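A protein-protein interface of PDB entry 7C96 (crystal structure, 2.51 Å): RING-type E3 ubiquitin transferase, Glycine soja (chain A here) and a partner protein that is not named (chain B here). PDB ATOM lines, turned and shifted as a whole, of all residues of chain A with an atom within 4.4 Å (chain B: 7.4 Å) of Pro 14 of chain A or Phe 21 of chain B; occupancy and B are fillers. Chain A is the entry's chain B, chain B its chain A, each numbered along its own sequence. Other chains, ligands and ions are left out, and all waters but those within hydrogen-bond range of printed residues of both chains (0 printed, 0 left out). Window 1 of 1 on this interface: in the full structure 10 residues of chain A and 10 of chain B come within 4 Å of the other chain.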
ATOM      1  N   ARG A  12     -13.965 -10.410 -29.894  1.00  0.00           N
ATOM      2  CA  ARG A  12     -12.633  -9.927 -30.218  1.00  0.00           C
ATOM      3  C   ARG A  12     -11.612 -10.516 -29.261  1.00  0.00           C
ATOM      4  O   ARG A  12     -11.892 -10.711 -28.076  1.00  0.00           O
ATOM      5  CB  ARG A  12     -12.554  -8.397 -30.172  1.00  0.00           C
ATOM      6  CG  ARG A  12     -13.434  -7.653 -31.170  1.00  0.00           C
ATOM      7  CD  ARG A  12     -13.333  -6.135 -30.960  1.00  0.00           C
ATOM      8  NE  ARG A  12     -14.237  -5.370 -31.828  1.00  0.00           N
ATOM      9  CZ  ARG A  12     -13.870  -4.814 -32.980  1.00  0.00           C
ATOM     10  NH1 ARG A  12     -14.743  -4.135 -33.711  1.00  0.00           N
ATOM     11  NH2 ARG A  12     -12.628  -4.945 -33.410  1.00  0.00           N
ATOM     12  N   CYS A  13     -10.439 -10.818 -29.795  1.00  0.00           N
ATOM     13  CA  CYS A  13      -9.339 -11.289 -28.966  1.00  0.00           C
ATOM     14  C   CYS A  13      -8.732 -10.118 -28.208  1.00  0.00           C
ATOM     15  O   CYS A  13      -8.449  -9.080 -28.811  1.00  0.00           O
ATOM     16  CB  CYS A  13      -8.259 -11.970 -29.809  1.00  0.00           C
ATOM     17  SG  CYS A  13      -6.760 -12.484 -28.899  1.00  0.00           S
ATOM     18  N   PRO A  14      -8.512 -10.250 -26.903  1.00  0.00           N
ATOM     19  CA  PRO A  14      -7.891  -9.150 -26.154  1.00  0.00           C
ATOM     20  C   PRO A  14      -6.536  -8.712 -26.700  1.00  0.00           C
ATOM     21  O   PRO A  14      -6.147  -7.562 -26.481  1.00  0.00           O
ATOM     22  CB  PRO A  14      -7.777  -9.725 -24.737  1.00  0.00           C
ATOM     23  CG  PRO A  14      -8.810 -10.785 -24.673  1.00  0.00           C
ATOM     24  CD  PRO A  14      -8.891 -11.377 -26.035  1.00  0.00           C
ATOM     25  N   ILE A  15      -5.802  -9.572 -27.395  1.00  0.00           N
ATOM     26  CA  ILE A  15      -4.489  -9.178 -27.913  1.00  0.00           C
ATOM     27  C   ILE A  15      -4.583  -8.674 -29.348  1.00  0.00           C
ATOM     28  O   ILE A  15      -4.063  -7.606 -29.674  1.00  0.00           O
ATOM     29  CB  ILE A  15      -3.511 -10.356 -27.803  1.00  0.00           C
ATOM     30  CG1 ILE A  15      -3.395 -10.790 -26.349  1.00  0.00           C
ATOM     31  CG2 ILE A  15      -2.165  -9.963 -28.322  1.00  0.00           C
ATOM     32  CD1 ILE A  15      -2.758 -12.128 -26.190  1.00  0.00           C
ATOM     33  N   SER A  16      -5.252  -9.422 -30.240  1.00  0.00           N
ATOM     34  CA  SER A  16      -5.374  -8.963 -31.626  1.00  0.00           C
ATOM     35  C   SER A  16      -6.349  -7.795 -31.753  1.00  0.00           C
ATOM     36  O   SER A  16      -6.231  -6.991 -32.681  1.00  0.00           O
ATOM     37  CB  SER A  16      -5.821 -10.097 -32.557  1.00  0.00           C
ATOM     38  OG  SER A  16      -7.041 -10.687 -32.173  1.00  0.00           O
ATOM     39  N   LEU A  17      -7.330  -7.712 -30.857  1.00  0.00           N
ATOM     40  CA  LEU A  17      -8.443  -6.768 -30.910  1.00  0.00           C
ATOM     41  C   LEU A  17      -9.298  -6.947 -32.157  1.00  0.00           C
ATOM     42  O   LEU A  17     -10.082  -6.054 -32.500  1.00  0.00           O
ATOM     43  CB  LEU A  17      -7.961  -5.315 -30.794  1.00  0.00           C
ATOM     44  CG  LEU A  17      -7.019  -5.105 -29.602  1.00  0.00           C
ATOM     45  CD1 LEU A  17      -6.310  -3.769 -29.699  1.00  0.00           C
ATOM     46  CD2 LEU A  17      -7.759  -5.270 -28.261  1.00  0.00           C
ATOM     47  N   THR A  31     -10.371 -16.245 -22.967  1.00  0.00           N
ATOM     48  CA  THR A  31     -10.334 -16.739 -24.332  1.00  0.00           C
ATOM     49  C   THR A  31      -9.499 -15.828 -25.211  1.00  0.00           C
ATOM     50  O   THR A  31      -9.593 -14.603 -25.113  1.00  0.00           O
ATOM     51  CB  THR A  31     -11.745 -16.872 -24.885  1.00  0.00           C
ATOM     52  OG1 THR A  31     -12.455 -17.778 -24.065  1.00  0.00           O
ATOM     53  CG2 THR A  31     -11.771 -17.380 -26.289  1.00  0.00           C
ATOM     54  N   TYR A  32      -8.690 -16.441 -26.074  1.00  0.00           N
ATOM     55  CA  TYR A  32      -7.764 -15.705 -26.912  1.00  0.00           C
ATOM     56  C   TYR A  32      -7.690 -16.368 -28.263  1.00  0.00           C
ATOM     57  O   TYR A  32      -8.039 -17.535 -28.420  1.00  0.00           O
ATOM     58  CB  TYR A  32      -6.360 -15.643 -26.353  1.00  0.00           C
ATOM     59  CG  TYR A  32      -6.266 -15.055 -24.985  1.00  0.00           C
ATOM     60  CD1 TYR A  32      -6.409 -15.857 -23.861  1.00  0.00           C
ATOM     61  CD2 TYR A  32      -5.984 -13.705 -24.801  1.00  0.00           C
ATOM     62  CE1 TYR A  32      -6.296 -15.330 -22.608  1.00  0.00           C
ATOM     63  CE2 TYR A  32      -5.851 -13.160 -23.530  1.00  0.00           C
ATOM     64  CZ  TYR A  32      -6.002 -13.978 -22.442  1.00  0.00           C
ATOM     65  OH  TYR A  32      -5.886 -13.472 -21.169  1.00  0.00           O
ATOM     66  N   PRO A  49      -2.638 -13.244 -20.037  1.00  0.00           N
ATOM     67  CA  PRO A  49      -2.397 -11.838 -20.403  1.00  0.00           C
ATOM     68  C   PRO A  49      -3.367 -10.872 -19.746  1.00  0.00           C
ATOM     69  O   PRO A  49      -2.948  -9.862 -19.174  1.00  0.00           O
ATOM     70  CB  PRO A  49      -2.552 -11.847 -21.931  1.00  0.00           C
ATOM     71  CG  PRO A  49      -2.274 -13.225 -22.331  1.00  0.00           C
ATOM     72  CD  PRO A  49      -2.729 -14.123 -21.206  1.00  0.00           C
ATOM     73  N   MET B  13       4.923  -1.505 -32.389  1.00  0.00           N
ATOM     74  CA  MET B  13       3.558  -1.842 -31.972  1.00  0.00           C
ATOM     75  C   MET B  13       2.653  -2.002 -33.189  1.00  0.00           C
ATOM     76  O   MET B  13       1.733  -2.817 -33.183  1.00  0.00           O
ATOM     77  CB  MET B  13       2.966  -0.785 -31.036  1.00  0.00           C
ATOM     78  CG  MET B  13       3.526  -0.802 -29.633  1.00  0.00           C
ATOM     79  SD  MET B  13       3.148   0.863 -28.646  1.00  0.00           S
ATOM     80  CE  MET B  13       1.210   0.914 -28.822  1.00  0.00           C
ATOM     81  N   ASP B  16       4.427  -5.673 -33.935  1.00  0.00           N
ATOM     82  CA  ASP B  16       4.182  -6.725 -32.949  1.00  0.00           C
ATOM     83  C   ASP B  16       2.898  -6.443 -32.175  1.00  0.00           C
ATOM     84  O   ASP B  16       2.719  -5.353 -31.623  1.00  0.00           O
ATOM     85  CB  ASP B  16       5.376  -6.851 -31.995  1.00  0.00           C
ATOM     86  CG  ASP B  16       5.324  -8.102 -31.130  1.00  0.00           C
ATOM     87  OD1 ASP B  16       4.273  -8.776 -31.046  1.00  0.00           O
ATOM     88  OD2 ASP B  16       6.353  -8.401 -30.495  1.00  0.00           O
ATOM     89  N   THR B  17       2.002  -7.426 -32.155  1.00  0.00           N
ATOM     90  CA  THR B  17       0.744  -7.286 -31.445  1.00  0.00           C
ATOM     91  C   THR B  17       0.914  -7.558 -29.954  1.00  0.00           C
ATOM     92  O   THR B  17       0.185  -6.986 -29.126  1.00  0.00           O
ATOM     93  CB  THR B  17      -0.299  -8.215 -32.093  1.00  0.00           C
ATOM     94  OG1 THR B  17      -1.620  -7.872 -31.657  1.00  0.00           O
ATOM     95  CG2 THR B  17      -0.035  -9.695 -31.789  1.00  0.00           C
ATOM     96  N   ILE B  18       1.874  -8.421 -29.605  1.00  0.00           N
ATOM     97  CA  ILE B  18       2.153  -8.733 -28.206  1.00  0.00           C
ATOM     98  C   ILE B  18       2.704  -7.504 -27.491  1.00  0.00           C
ATOM     99  O   ILE B  18       2.191  -7.081 -26.450  1.00  0.00           O
ATOM    100  CB  ILE B  18       3.130  -9.921 -28.119  1.00  0.00           C
ATOM    101  CG1 ILE B  18       2.546 -11.189 -28.765  1.00  0.00           C
ATOM    102  CG2 ILE B  18       3.579 -10.185 -26.695  1.00  0.00           C
ATOM    103  CD1 ILE B  18       1.203 -11.673 -28.264  1.00  0.00           C
ATOM    104  N   LEU B  19       3.748  -6.898 -28.056  1.00  0.00           N
ATOM    105  CA  LEU B  19       4.284  -5.676 -27.477  1.00  0.00           C
ATOM    106  C   LEU B  19       3.208  -4.596 -27.403  1.00  0.00           C
ATOM    107  O   LEU B  19       3.100  -3.881 -26.397  1.00  0.00           O
ATOM    108  CB  LEU B  19       5.493  -5.205 -28.292  1.00  0.00           C
ATOM    109  CG  LEU B  19       6.276  -4.003 -27.727  1.00  0.00           C
ATOM    110  CD1 LEU B  19       7.437  -4.471 -26.875  1.00  0.00           C
ATOM    111  CD2 LEU B  19       6.777  -3.067 -28.818  1.00  0.00           C
ATOM    112  N   ARG B  20       2.386  -4.480 -28.452  1.00  0.00           N
ATOM    113  CA  ARG B  20       1.358  -3.440 -28.492  1.00  0.00           C
ATOM    114  C   ARG B  20       0.345  -3.631 -27.372  1.00  0.00           C
ATOM    115  O   ARG B  20      -0.139  -2.661 -26.782  1.00  0.00           O
ATOM    116  CB  ARG B  20       0.676  -3.438 -29.867  1.00  0.00           C
ATOM    117  CG  ARG B  20      -0.441  -2.415 -30.075  1.00  0.00           C
ATOM    118  CD  ARG B  20      -1.744  -3.150 -30.287  1.00  0.00           C
ATOM    119  NE  ARG B  20      -2.224  -3.244 -31.675  1.00  0.00           N
ATOM    120  CZ  ARG B  20      -3.202  -4.072 -32.070  1.00  0.00           C
ATOM    121  NH1 ARG B  20      -3.747  -4.908 -31.207  1.00  0.00           N
ATOM    122  NH2 ARG B  20      -3.618  -4.109 -33.330  1.00  0.00           N
ATOM    123  N   PHE B  21      -0.003  -4.877 -27.074  1.00  0.00           N
ATOM    124  CA  PHE B  21      -0.909  -5.126 -25.963  1.00  0.00           C
ATOM    125  C   PHE B  21      -0.243  -4.810 -24.623  1.00  0.00           C
ATOM    126  O   PHE B  21      -0.893  -4.285 -23.712  1.00  0.00           O
ATOM    127  CB  PHE B  21      -1.406  -6.567 -26.013  1.00  0.00           C
ATOM    128  CG  PHE B  21      -2.084  -7.013 -24.760  1.00  0.00           C
ATOM    129  CD1 PHE B  21      -3.394  -6.648 -24.500  1.00  0.00           C
ATOM    130  CD2 PHE B  21      -1.414  -7.793 -23.834  1.00  0.00           C
ATOM    131  CE1 PHE B  21      -4.034  -7.062 -23.315  1.00  0.00           C
ATOM    132  CE2 PHE B  21      -2.040  -8.207 -22.656  1.00  0.00           C
ATOM    133  CZ  PHE B  21      -3.355  -7.841 -22.395  1.00  0.00           C
ATOM    134  N   GLN B  22       1.048  -5.117 -24.479  1.00  0.00           N
ATOM    135  CA  GLN B  22       1.732  -4.820 -23.224  1.00  0.00           C
ATOM    136  C   GLN B  22       1.700  -3.330 -22.937  1.00  0.00           C
ATOM    137  O   GLN B  22       1.373  -2.896 -21.822  1.00  0.00           O
ATOM    138  CB  GLN B  22       3.169  -5.323 -23.280  1.00  0.00           C
ATOM    139  CG  GLN B  22       3.229  -6.823 -23.259  1.00  0.00           C
ATOM    140  CD  GLN B  22       4.638  -7.363 -23.231  1.00  0.00           C
ATOM    141  OE1 GLN B  22       5.369  -7.305 -24.231  1.00  0.00           O
ATOM    142  NE2 GLN B  22       5.024  -7.929 -22.091  1.00  0.00           N
ATOM    143  N   MET B  23       2.013  -2.535 -23.951  1.00  0.00           N
ATOM    144  CA  MET B  23       2.022  -1.095 -23.874  1.00  0.00           C
ATOM    145  C   MET B  23       0.613  -0.550 -23.634  1.00  0.00           C
ATOM    146  O   MET B  23       0.427   0.405 -22.878  1.00  0.00           O
ATOM    147  CB  MET B  23       2.619  -0.527 -25.162  1.00  0.00           C
ATOM    148  CG  MET B  23       4.157  -0.670 -25.294  1.00  0.00           C
ATOM    149  SD  MET B  23       5.354  -0.347 -23.741  1.00  0.00           S
ATOM    150  CE  MET B  23       6.323  -2.069 -23.678  1.00  0.00           C
ATOM    151  N   PHE B  24      -0.382  -1.166 -24.278  1.00  0.00           N
ATOM    152  CA  PHE B  24      -1.767  -0.756 -24.061  1.00  0.00           C
ATOM    153  C   PHE B  24      -2.182  -0.980 -22.609  1.00  0.00           C
ATOM    154  O   PHE B  24      -2.918  -0.168 -22.031  1.00  0.00           O
ATOM    155  CB  PHE B  24      -2.686  -1.508 -25.019  1.00  0.00           C
ATOM    156  CG  PHE B  24      -2.803  -0.873 -26.383  1.00  0.00           C
ATOM    157  CD1 PHE B  24      -2.048   0.242 -26.723  1.00  0.00           C
ATOM    158  CD2 PHE B  24      -3.645  -1.425 -27.344  1.00  0.00           C
ATOM    159  CE1 PHE B  24      -2.154   0.809 -27.988  1.00  0.00           C
ATOM    160  CE2 PHE B  24      -3.764  -0.863 -28.599  1.00  0.00           C
ATOM    161  CZ  PHE B  24      -3.015   0.265 -28.921  1.00  0.00           C
ATOM    162  N   THR B  25      -1.705  -2.065 -21.993  1.00  0.00           N
ATOM    163  CA  THR B  25      -2.001  -2.275 -20.579  1.00  0.00           C
ATOM    164  C   THR B  25      -1.319  -1.220 -19.722  1.00  0.00           C
ATOM    165  O   THR B  25      -1.821  -0.873 -18.646  1.00  0.00           O
ATOM    166  CB  THR B  25      -1.575  -3.676 -20.122  1.00  0.00           C
ATOM    167  OG1 THR B  25      -1.756  -4.616 -21.184  1.00  0.00           O
ATOM    168  CG2 THR B  25      -2.417  -4.129 -18.931  1.00  0.00           C
ATOM    169  N   LYS B  26      -0.171  -0.716 -20.168  1.00  0.00           N
ATOM    170  CA  LYS B  26       0.515   0.309 -19.399  1.00  0.00           C
ATOM    171  C   LYS B  26      -0.160   1.667 -19.555  1.00  0.00           C
ATOM    172  O   LYS B  26      -0.334   2.393 -18.569  1.00  0.00           O
ATOM    173  CB  LYS B  26       1.979   0.369 -19.824  1.00  0.00           C
ATOM    174  CG  LYS B  26       2.896  -0.540 -19.015  1.00  0.00           C
ATOM    175  CD  LYS B  26       4.266  -0.652 -19.680  1.00  0.00           C
ATOM    176  CE  LYS B  26       4.984  -1.940 -19.304  1.00  0.00           C
ATOM    177  NZ  LYS B  26       6.273  -1.632 -18.611  1.00  0.00           N
ATOM    178  N   TRP B  27      -0.554   2.020 -20.781  1.00  0.00           N
ATOM    179  CA  TRP B  27      -1.283   3.265 -21.004  1.00  0.00           C
ATOM    180  C   TRP B  27      -2.612   3.281 -20.252  1.00  0.00           C
ATOM    181  O   TRP B  27      -3.016   4.317 -19.708  1.00  0.00           O
ATOM    182  CB  TRP B  27      -1.532   3.464 -22.497  1.00  0.00           C
ATOM    183  CG  TRP B  27      -0.307   3.563 -23.379  1.00  0.00           C
ATOM    184  CD1 TRP B  27       1.004   3.455 -23.009  1.00  0.00           C
ATOM    185  CD2 TRP B  27      -0.304   3.797 -24.791  1.00  0.00           C
ATOM    186  NE1 TRP B  27       1.823   3.610 -24.108  1.00  0.00           N
ATOM    187  CE2 TRP B  27       1.041   3.823 -25.210  1.00  0.00           C
ATOM    188  CE3 TRP B  27      -1.310   3.986 -25.737  1.00  0.00           C
ATOM    189  CZ2 TRP B  27       1.399   4.028 -26.529  1.00  0.00           C
ATOM    190  CZ3 TRP B  27      -0.955   4.197 -27.037  1.00  0.00           C
ATOM    191  CH2 TRP B  27       0.390   4.217 -27.428  1.00  0.00           C
ATOM    192  N   HIS B  52      -9.112  -1.221 -27.206  1.00  0.00           N
ATOM    193  CA  HIS B  52      -8.489  -1.784 -26.011  1.00  0.00           C
ATOM    194  C   HIS B  52      -9.033  -1.145 -24.732  1.00  0.00           C
ATOM    195  O   HIS B  52      -9.244  -1.839 -23.729  1.00  0.00           O
ATOM    196  CB  HIS B  52      -6.971  -1.628 -26.089  1.00  0.00           C
ATOM    197  CG  HIS B  52      -6.241  -2.290 -24.965  1.00  0.00           C
ATOM    198  ND1 HIS B  52      -6.096  -1.701 -23.728  1.00  0.00           N
ATOM    199  CD2 HIS B  52      -5.592  -3.477 -24.897  1.00  0.00           C
ATOM    200  CE1 HIS B  52      -5.406  -2.504 -22.941  1.00  0.00           C
ATOM    201  NE2 HIS B  52      -5.086  -3.589 -23.625  1.00  0.00           N
ATOM    202  N   MET B  55     -12.767  -2.512 -23.920  1.00  0.00           N
ATOM    203  CA  MET B  55     -12.982  -3.879 -23.445  1.00  0.00           C
ATOM    204  C   MET B  55     -11.959  -4.390 -22.426  1.00  0.00           C
ATOM    205  O   MET B  55     -12.213  -5.392 -21.744  1.00  0.00           O
ATOM    206  CB  MET B  55     -13.024  -4.843 -24.631  1.00  0.00           C
ATOM    207  CG  MET B  55     -11.675  -5.262 -25.162  1.00  0.00           C
ATOM    208  SD  MET B  55     -11.821  -6.308 -26.805  1.00  0.00           S
ATOM    209  CE  MET B  55     -12.363  -8.065 -26.048  1.00  0.00           C
ATOM    210  N   ASN B  56     -10.805  -3.736 -22.332  1.00  0.00           N
ATOM    211  CA  ASN B  56      -9.843  -4.048 -21.279  1.00  0.00           C
ATOM    212  C   ASN B  56      -9.830  -2.907 -20.273  1.00  0.00           C
ATOM    213  O   ASN B  56     -10.879  -2.493 -19.770  1.00  0.00           O
ATOM    214  CB  ASN B  56      -8.436  -4.277 -21.845  1.00  0.00           C
ATOM    215  CG  ASN B  56      -8.316  -5.579 -22.620  1.00  0.00           C
ATOM    216  OD1 ASN B  56      -9.132  -6.485 -22.452  1.00  0.00           O
ATOM    217  ND2 ASN B  56      -7.298  -5.680 -23.472  1.00  0.00           N
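OG1 of Thr 17 of chain B sits at hydrogen-bond distance from O of Ile 15 of chain A, at 3.2 Å.
The guanidinium group of Arg 20 of chain B is in hydrogen-bond range of the backbone carbonyl oxygen of Ile 15 of chain A.
The backbone NH (N) of Ile 18 of chain B sits at hydrogen-bond distance from the side-chain carboxylate (OD1) of Asp 16 of chain B (2.8 Å).
The backbone carbonyl oxygen of Phe 21 of chain B sits at hydrogen-bond distance from the side-chain hydroxyl of Thr 25 of chain B, at 2.7 Å.
A ring nitrogen (NE2) of His 52 of chain B lies within hydrogen-bond range of the side-chain amide nitrogen (ND2) of Asn 56 of chain B (3.0 Å).
The backbone carbonyl oxygen (O) of Leu 17 of chain A sits at hydrogen-bond distance from the guanidinium group (NH2) of Arg 12 of chain A (2.9 Å).
The backbone NH (N) of Ile 15 of chain A lies close to the side-chain sulfur (SG) of Cys 13 of chain A (3.4 Å).
The side-chain sulfur (SG) of Cys 13 of chain A lies within hydrogen-bond range of the backbone NH (N) of Ser 16 of chain A, 3.7 Å away.
Among the printed residues, merely in contact across the chains: Arg 12 of chain A with Met 55 of chain B, Pro 14 of chain A with Phe 21 of chain B, Pro 14 of chain A with Asn 56 of chain B, Ile 15 of chain A with Ile 18 of chain B, Ser 16 of chain A with Thr 17 of chain B, Ser 16 of chain A with Arg 20 of chain B, Leu 17 of chain A with Arg 20 of chain B and Pro 49 of chain A with Phe 21 of chain B.
Printed residues of chain B within 4 Å of Pro 14 of chain A: Phe 21 and Asn 56.
Phe 21 of chain B touches just these residues of chain A: Pro 14 (3.5 Å) and Pro 49 (3.7 Å).
Of the printed residues of chain B, Leu 17 of chain A touches Arg 20 (3.2 Å).
Of the printed residues of chain B, Ser 16 of chain A touches Thr 17 (3.9 Å) and Arg 20 (3.6 Å).
Printed residues of chain A within 4 Å of Arg 20 of chain B: Ile 15 (3.1 Å), Ser 16 (3.6 Å) and Leu 17 (3.2 Å).
The nearest residue of chain B that does not touch Pro 14 of chain A is His 52 of chain B (4.4 Å).
The nearest printed residue of chain B that does not touch Ser 16 of chain A is Phe 21 of chain B (6.4 Å).
Of the 9 printed residues of chain A, 6 touch a printed residue of chain B.
Hydrophobic or aromatic side chains of chain A within 4 Å of the printed part of chain B: Ile 15, Leu 17 and Pro 49.
Of the 16 printed residues of chain B, 6 touch a printed residue of chain A.
Hydrophobic or aromatic side chains of chain B within 4 Å of the printed part of chain A: Ile 18, Phe 21 and Met 55.
Along chain B the printed residues that touch a printed residue of chain A span positions 17 to 56.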
